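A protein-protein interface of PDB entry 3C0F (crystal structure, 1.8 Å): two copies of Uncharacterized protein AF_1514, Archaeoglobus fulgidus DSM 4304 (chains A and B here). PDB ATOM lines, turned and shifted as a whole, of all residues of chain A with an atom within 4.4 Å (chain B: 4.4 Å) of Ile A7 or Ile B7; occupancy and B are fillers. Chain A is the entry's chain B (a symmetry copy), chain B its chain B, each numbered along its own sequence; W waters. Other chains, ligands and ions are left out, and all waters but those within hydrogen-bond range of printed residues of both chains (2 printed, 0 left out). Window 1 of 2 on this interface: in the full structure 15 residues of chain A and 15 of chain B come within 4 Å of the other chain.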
ATOM      1  N   GLU A   6       2.348 -20.270 -23.002  1.00  0.00           N
ATOM      2  CA  GLU A   6       3.210 -19.524 -23.920  1.00  0.00           C
ATOM      3  C   GLU A   6       2.413 -18.650 -24.880  1.00  0.00           C
ATOM      4  O   GLU A   6       1.350 -19.042 -25.362  1.00  0.00           O
ATOM      5  CB  GLU A   6       4.095 -20.482 -24.728  1.00  0.00           C
ATOM      6  CG  GLU A   6       5.118 -21.251 -23.909  1.00  0.00           C
ATOM      7  CD  GLU A   6       5.977 -22.184 -24.751  1.00  0.00           C
ATOM      8  OE1 GLU A   6       6.027 -22.019 -25.989  1.00  0.00           O
ATOM      9  OE2 GLU A   6       6.612 -23.084 -24.164  1.00  0.00           O
ATOM     10  N   ILE A   7       2.944 -17.464 -25.154  1.00  0.00           N
ATOM     11  CA  ILE A   7       2.382 -16.572 -26.166  1.00  0.00           C
ATOM     12  C   ILE A   7       3.530 -16.133 -27.071  1.00  0.00           C
ATOM     13  O   ILE A   7       4.530 -15.585 -26.597  1.00  0.00           O
ATOM     14  CB  ILE A   7       1.658 -15.349 -25.530  1.00  0.00           C
ATOM     15  CG1 ILE A   7       0.474 -15.811 -24.664  1.00  0.00           C
ATOM     16  CG2 ILE A   7       1.182 -14.367 -26.614  1.00  0.00           C
ATOM     17  CD1 ILE A   7      -0.163 -14.727 -23.793  1.00  0.00           C
ATOM     18  N   MLY A   8       3.399 -16.404 -28.366  1.00  0.00           N
ATOM     19  CA  MLY A   8       4.446 -16.069 -29.327  1.00  0.00           C
ATOM     20  CB  MLY A   8       4.951 -17.324 -30.036  1.00  0.00           C
ATOM     21  CG  MLY A   8       6.004 -17.014 -31.099  1.00  0.00           C
ATOM     22  CD  MLY A   8       6.615 -18.299 -31.644  1.00  0.00           C
ATOM     23  CE  MLY A   8       7.697 -18.032 -32.693  1.00  0.00           C
ATOM     24  NZ  MLY A   8       8.796 -17.200 -32.164  1.00  0.00           N
ATOM     25  CH1 MLY A   8       9.554 -16.637 -33.290  1.00  0.00           C
ATOM     26  CH2 MLY A   8       9.710 -18.008 -31.336  1.00  0.00           C
ATOM     27  C   MLY A   8       3.932 -15.057 -30.301  1.00  0.00           C
ATOM     28  O   MLY A   8       2.996 -15.329 -31.052  1.00  0.00           O
ATOM     29  N   VAL A   9       4.554 -13.881 -30.290  1.00  0.00           N
ATOM     30  CA  VAL A   9       4.165 -12.775 -31.160  1.00  0.00           C
ATOM     31  C   VAL A   9       5.178 -12.620 -32.296  1.00  0.00           C
ATOM     32  O   VAL A   9       6.383 -12.529 -32.056  1.00  0.00           O
ATOM     33  CB  VAL A   9       4.041 -11.448 -30.370  1.00  0.00           C
ATOM     34  CG1 VAL A   9       3.554 -10.324 -31.274  1.00  0.00           C
ATOM     35  CG2 VAL A   9       3.103 -11.617 -29.172  1.00  0.00           C
ATOM     36  N   ILE A  27       0.554  -7.439 -23.018  1.00  0.00           N
ATOM     37  CA  ILE A  27      -0.139  -8.728 -23.113  1.00  0.00           C
ATOM     38  C   ILE A  27      -0.290  -9.395 -21.743  1.00  0.00           C
ATOM     39  O   ILE A  27      -1.392  -9.816 -21.378  1.00  0.00           O
ATOM     40  CB  ILE A  27       0.561  -9.687 -24.105  1.00  0.00           C
ATOM     41  CG1 ILE A  27       0.389  -9.179 -25.541  1.00  0.00           C
ATOM     42  CG2 ILE A  27      -0.003 -11.106 -23.978  1.00  0.00           C
ATOM     43  CD1 ILE A  27       1.360  -9.788 -26.535  1.00  0.00           C
ATOM     44  N   TYR A  31      -3.748 -10.757 -17.683  1.00  0.00           N
ATOM     45  CA  TYR A  31      -3.861 -11.982 -16.880  1.00  0.00           C
ATOM     46  C   TYR A  31      -3.580 -11.778 -15.395  1.00  0.00           C
ATOM     47  O   TYR A  31      -3.890 -12.641 -14.570  1.00  0.00           O
ATOM     48  CB  TYR A  31      -2.983 -13.085 -17.485  1.00  0.00           C
ATOM     49  CG  TYR A  31      -3.195 -13.191 -18.978  1.00  0.00           C
ATOM     50  CD1 TYR A  31      -4.428 -13.594 -19.496  1.00  0.00           C
ATOM     51  CD2 TYR A  31      -2.184 -12.838 -19.871  1.00  0.00           C
ATOM     52  CE1 TYR A  31      -4.642 -13.670 -20.868  1.00  0.00           C
ATOM     53  CE2 TYR A  31      -2.386 -12.913 -21.251  1.00  0.00           C
ATOM     54  CZ  TYR A  31      -3.616 -13.328 -21.740  1.00  0.00           C
ATOM     55  OH  TYR A  31      -3.826 -13.401 -23.096  1.00  0.00           O
ATOM     56  N   LEU A  70       4.372 -17.814 -17.325  1.00  0.00           N
ATOM     57  CA  LEU A  70       4.008 -17.325 -18.656  1.00  0.00           C
ATOM     58  C   LEU A  70       5.231 -16.848 -19.434  1.00  0.00           C
ATOM     59  O   LEU A  70       5.957 -15.956 -18.987  1.00  0.00           O
ATOM     60  CB  LEU A  70       2.959 -16.208 -18.572  1.00  0.00           C
ATOM     61  CG  LEU A  70       2.416 -15.622 -19.885  1.00  0.00           C
ATOM     62  CD1 LEU A  70       1.698 -16.666 -20.746  1.00  0.00           C
ATOM     63  CD2 LEU A  70       1.491 -14.453 -19.589  1.00  0.00           C
ATOM     64  N   MLY A  71       5.443 -17.461 -20.594  1.00  0.00           N
ATOM     65  CA  MLY A  71       6.506 -17.069 -21.510  1.00  0.00           C
ATOM     66  CB  MLY A  71       7.193 -18.337 -22.007  1.00  0.00           C
ATOM     67  CG  MLY A  71       8.259 -18.079 -23.065  1.00  0.00           C
ATOM     68  CD  MLY A  71       8.610 -19.384 -23.773  1.00  0.00           C
ATOM     69  CE  MLY A  71       9.869 -19.225 -24.618  1.00  0.00           C
ATOM     70  NZ  MLY A  71      10.220 -20.479 -25.315  1.00  0.00           N
ATOM     71  CH1 MLY A  71      10.745 -21.480 -24.375  1.00  0.00           C
ATOM     72  CH2 MLY A  71      11.265 -20.192 -26.304  1.00  0.00           C
ATOM     73  C   MLY A  71       5.915 -16.306 -22.659  1.00  0.00           C
ATOM     74  O   MLY A  71       5.034 -16.811 -23.354  1.00  0.00           O
ATOM     75  N   ILE A  72       6.385 -15.079 -22.866  1.00  0.00           N
ATOM     76  CA  ILE A  72       5.932 -14.275 -24.003  1.00  0.00           C
ATOM     77  C   ILE A  72       7.112 -13.947 -24.912  1.00  0.00           C
ATOM     78  O   ILE A  72       8.084 -13.317 -24.481  1.00  0.00           O
ATOM     79  CB  ILE A  72       5.207 -12.969 -23.572  1.00  0.00           C
ATOM     80  CG1 ILE A  72       3.976 -13.287 -22.708  1.00  0.00           C
ATOM     81  CG2 ILE A  72       4.815 -12.141 -24.810  1.00  0.00           C
ATOM     82  CD1 ILE A  72       3.349 -12.070 -22.039  1.00  0.00           C
ATOM     83  N   SER A  73       7.030 -14.397 -26.160  1.00  0.00           N
ATOM     84  CA  SER A  73       8.040 -14.056 -27.159  1.00  0.00           C
ATOM     85  C   SER A  73       7.522 -12.956 -28.075  1.00  0.00           C
ATOM     86  O   SER A  73       6.361 -12.983 -28.495  1.00  0.00           O
ATOM     87  CB  SER A  73       8.454 -15.285 -27.977  1.00  0.00           C
ATOM     88  OG  SER A  73       9.061 -16.269 -27.153  1.00  0.00           O
ATOM     89  N   GLU B   6       1.069 -11.828 -36.310  1.00  0.00           N
ATOM     90  CA  GLU B   6       0.550 -13.073 -35.741  1.00  0.00           C
ATOM     91  C   GLU B   6       0.822 -13.184 -34.246  1.00  0.00           C
ATOM     92  O   GLU B   6       1.883 -12.790 -33.763  1.00  0.00           O
ATOM     93  CB  GLU B   6       1.160 -14.288 -36.454  1.00  0.00           C
ATOM     94  CG  GLU B   6       0.767 -14.434 -37.915  1.00  0.00           C
ATOM     95  CD  GLU B   6       1.389 -15.654 -38.581  1.00  0.00           C
ATOM     96  OE1 GLU B   6       1.856 -16.569 -37.868  1.00  0.00           O
ATOM     97  OE2 GLU B   6       1.403 -15.696 -39.828  1.00  0.00           O
ATOM     98  N   ILE B   7      -0.150 -13.730 -33.524  1.00  0.00           N
ATOM     99  CA  ILE B   7       0.013 -14.042 -32.106  1.00  0.00           C
ATOM    100  C   ILE B   7      -0.445 -15.484 -31.903  1.00  0.00           C
ATOM    101  O   ILE B   7      -1.579 -15.836 -32.241  1.00  0.00           O
ATOM    102  CB  ILE B   7      -0.782 -13.058 -31.196  1.00  0.00           C
ATOM    103  CG1 ILE B   7      -0.269 -11.620 -31.378  1.00  0.00           C
ATOM    104  CG2 ILE B   7      -0.691 -13.480 -29.720  1.00  0.00           C
ATOM    105  CD1 ILE B   7      -1.127 -10.533 -30.729  1.00  0.00           C
ATOM    106  N   MLY B   8       0.448 -16.320 -31.384  1.00  0.00           N
ATOM    107  CA  MLY B   8       0.143 -17.734 -31.178  1.00  0.00           C
ATOM    108  CB  MLY B   8       1.109 -18.616 -31.966  1.00  0.00           C
ATOM    109  CG  MLY B   8       0.869 -20.106 -31.731  1.00  0.00           C
ATOM    110  CD  MLY B   8       1.720 -20.946 -32.674  1.00  0.00           C
ATOM    111  CE  MLY B   8       1.488 -22.448 -32.489  1.00  0.00           C
ATOM    112  NZ  MLY B   8       0.077 -22.825 -32.700  1.00  0.00           N
ATOM    113  CH1 MLY B   8      -0.158 -24.149 -32.107  1.00  0.00           C
ATOM    114  CH2 MLY B   8      -0.238 -22.889 -34.139  1.00  0.00           C
ATOM    115  C   MLY B   8       0.178 -18.050 -29.716  1.00  0.00           C
ATOM    116  O   MLY B   8       1.223 -17.935 -29.076  1.00  0.00           O
ATOM    117  N   VAL B   9      -0.974 -18.456 -29.189  1.00  0.00           N
ATOM    118  CA  VAL B   9      -1.120 -18.784 -27.774  1.00  0.00           C
ATOM    119  C   VAL B   9      -1.195 -20.301 -27.591  1.00  0.00           C
ATOM    120  O   VAL B   9      -2.001 -20.973 -28.238  1.00  0.00           O
ATOM    121  CB  VAL B   9      -2.373 -18.110 -27.162  1.00  0.00           C
ATOM    122  CG1 VAL B   9      -2.465 -18.392 -25.669  1.00  0.00           C
ATOM    123  CG2 VAL B   9      -2.358 -16.601 -27.422  1.00  0.00           C
ATOM    124  N   ILE B  27      -6.985 -10.350 -26.270  1.00  0.00           N
ATOM    125  CA  ILE B  27      -5.677  -9.955 -26.801  1.00  0.00           C
ATOM    126  C   ILE B  27      -5.804  -8.885 -27.889  1.00  0.00           C
ATOM    127  O   ILE B  27      -5.117  -7.859 -27.831  1.00  0.00           O
ATOM    128  CB  ILE B  27      -4.881 -11.171 -27.333  1.00  0.00           C
ATOM    129  CG1 ILE B  27      -4.442 -12.065 -26.167  1.00  0.00           C
ATOM    130  CG2 ILE B  27      -3.657 -10.710 -28.132  1.00  0.00           C
ATOM    131  CD1 ILE B  27      -4.030 -13.466 -26.582  1.00  0.00           C
ATOM    132  N   TYR B  31      -5.052  -3.590 -29.195  1.00  0.00           N
ATOM    133  CA  TYR B  31      -4.529  -2.961 -30.414  1.00  0.00           C
ATOM    134  C   TYR B  31      -5.546  -2.095 -31.150  1.00  0.00           C
ATOM    135  O   TYR B  31      -5.186  -1.305 -32.026  1.00  0.00           O
ATOM    136  CB  TYR B  31      -3.914  -4.027 -31.329  1.00  0.00           C
ATOM    137  CG  TYR B  31      -2.997  -4.946 -30.554  1.00  0.00           C
ATOM    138  CD1 TYR B  31      -1.821  -4.459 -29.977  1.00  0.00           C
ATOM    139  CD2 TYR B  31      -3.329  -6.285 -30.351  1.00  0.00           C
ATOM    140  CE1 TYR B  31      -0.984  -5.289 -29.239  1.00  0.00           C
ATOM    141  CE2 TYR B  31      -2.495  -7.129 -29.616  1.00  0.00           C
ATOM    142  CZ  TYR B  31      -1.327  -6.623 -29.063  1.00  0.00           C
ATOM    143  OH  TYR B  31      -0.501  -7.444 -28.333  1.00  0.00           O
ATOM    144  N   LEU B  70      -4.487  -9.154 -38.392  1.00  0.00           N
ATOM    145  CA  LEU B  70      -3.987  -9.839 -37.199  1.00  0.00           C
ATOM    146  C   LEU B  70      -4.573 -11.242 -37.069  1.00  0.00           C
ATOM    147  O   LEU B  70      -5.793 -11.416 -37.014  1.00  0.00           O
ATOM    148  CB  LEU B  70      -4.268  -9.024 -35.929  1.00  0.00           C
ATOM    149  CG  LEU B  70      -3.753  -9.568 -34.588  1.00  0.00           C
ATOM    150  CD1 LEU B  70      -2.227  -9.699 -34.550  1.00  0.00           C
ATOM    151  CD2 LEU B  70      -4.239  -8.688 -33.448  1.00  0.00           C
ATOM    152  N   MLY B  71      -3.684 -12.229 -37.031  1.00  0.00           N
ATOM    153  CA  MLY B  71      -4.059 -13.620 -36.814  1.00  0.00           C
ATOM    154  CB  MLY B  71      -3.283 -14.479 -37.807  1.00  0.00           C
ATOM    155  CG  MLY B  71      -3.496 -15.975 -37.617  1.00  0.00           C
ATOM    156  CD  MLY B  71      -2.416 -16.750 -38.366  1.00  0.00           C
ATOM    157  CE  MLY B  71      -2.764 -18.232 -38.447  1.00  0.00           C
ATOM    158  NZ  MLY B  71      -1.726 -18.998 -39.165  1.00  0.00           N
ATOM    159  CH1 MLY B  71      -1.757 -18.713 -40.607  1.00  0.00           C
ATOM    160  CH2 MLY B  71      -1.981 -20.430 -38.979  1.00  0.00           C
ATOM    161  C   MLY B  71      -3.723 -14.011 -35.405  1.00  0.00           C
ATOM    162  O   MLY B  71      -2.573 -13.899 -34.985  1.00  0.00           O
ATOM    163  N   ILE B  72      -4.725 -14.466 -34.657  1.00  0.00           N
ATOM    164  CA  ILE B  72      -4.496 -14.945 -33.292  1.00  0.00           C
ATOM    165  C   ILE B  72      -4.891 -16.414 -33.183  1.00  0.00           C
ATOM    166  O   ILE B  72      -6.047 -16.777 -33.426  1.00  0.00           O
ATOM    167  CB  ILE B  72      -5.247 -14.105 -32.221  1.00  0.00           C
ATOM    168  CG1 ILE B  72      -4.811 -12.632 -32.276  1.00  0.00           C
ATOM    169  CG2 ILE B  72      -5.017 -14.698 -30.818  1.00  0.00           C
ATOM    170  CD1 ILE B  72      -5.668 -11.694 -31.434  1.00  0.00           C
ATOM    171  N   SER B  73      -3.920 -17.255 -32.839  1.00  0.00           N
ATOM    172  CA  SER B  73      -4.193 -18.668 -32.591  1.00  0.00           C
ATOM    173  C   SER B  73      -4.245 -18.939 -31.094  1.00  0.00           C
ATOM    174  O   SER B  73      -3.419 -18.426 -30.334  1.00  0.00           O
ATOM    175  CB  SER B  73      -3.143 -19.565 -33.262  1.00  0.00           C
ATOM    176  OG  SER B  73      -3.173 -19.420 -34.674  1.00  0.00           O
HETATM  177  O   HOH W   1       3.014 -19.975 -28.285  1.00  0.00           O
HETATM  178  O   HOH W   2       3.111 -16.057 -33.783  1.00  0.00           O
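O of MLY A8 lies within hydrogen-bond range of N of MLY B8.
The backbone NH (N) of Ile B7 is in hydrogen-bond range of O of MLY B71, at 2.8 Å.
O of Ile B7 lies within hydrogen-bond range of N of Ser B73, at 2.8 Å.
N of Val B9 lies within hydrogen-bond range of O of Ser B73 (2.7 Å).
O of MLY A71 sits at hydrogen-bond distance from the backbone NH (N) of Ile A7, 2.8 Å away.
N of Ser A73 sits at hydrogen-bond distance from O of Ile A7, 2.8 Å away.
N of Val A9 sits at hydrogen-bond distance from O of Ser A73, 2.7 Å away.
O of Glu A6 touches O of MLY B8 (3.9 Å).
Glu A6 touches Val B9.
Ile A7 touches Ile B7 (CG2 to CG2, 3.7 Å).
Ile A7 touches MLY B8 (CA to O, 3.4 Å).
Glu B6 touches MLY A8 (O to O, 3.9 Å).
O of MLY A8 touches CA of Ile B7, 3.4 Å away.
O of Glu B6 touches CA of Val A9, 3.5 Å away.
Tyr B31 touches Ile A27 (OH to CG1, 3.4 Å).
Ile B27 touches Tyr A31.
Of the printed residues of chain B, Glu A6 touches MLY B8 (3.9 Å) and Val B9 (3.5 Å).
Of the printed residues of chain B, Ile A7 touches Ile B7 and MLY B8.
Printed residues of chain B within 4 Å of Val A9: Glu B6 (3.5 Å).
Of chain A, only Ile A7 and MLY A8 come within 4 Å of Ile B7.
Printed residues of chain A within 4 Å of Val B9: Glu A6 (3.5 Å).
Leu B70 touches none of the printed residues of chain A.
Ile B72 touches none of the printed residues of chain A.
The nearest printed residue of chain A that does not touch MLY B8 is Val A9 (4.9 Å).
Of the 10 printed residues of chain B, 6 touch a printed residue of chain A.
Among the printed residues, no Asp or Glu carboxylate lies within 4 Å of a Lys or Arg side-chain nitrogen of the other chain.
Glu A6 touches MLY B8, and with the chains exchanged MLY A8 touches Glu B6.
Glu A6 touches Val B9, and with the chains exchanged Val A9 touches Glu B6.
Ile A7 touches MLY B8, and with the chains exchanged MLY A8 touches Ile B7.
MLY A8 touches its own counterpart, MLY B8.
Positions printed for both chains: 6, 7, 8, 9, 27, 31, 70, 71, 72 and 73.
Water W1 bridges O of MLY B8 and the backbone carbonyl oxygen (O) of Glu A6.
Water W2 bridges O of MLY A8 and the backbone carbonyl oxygen of Glu B6.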
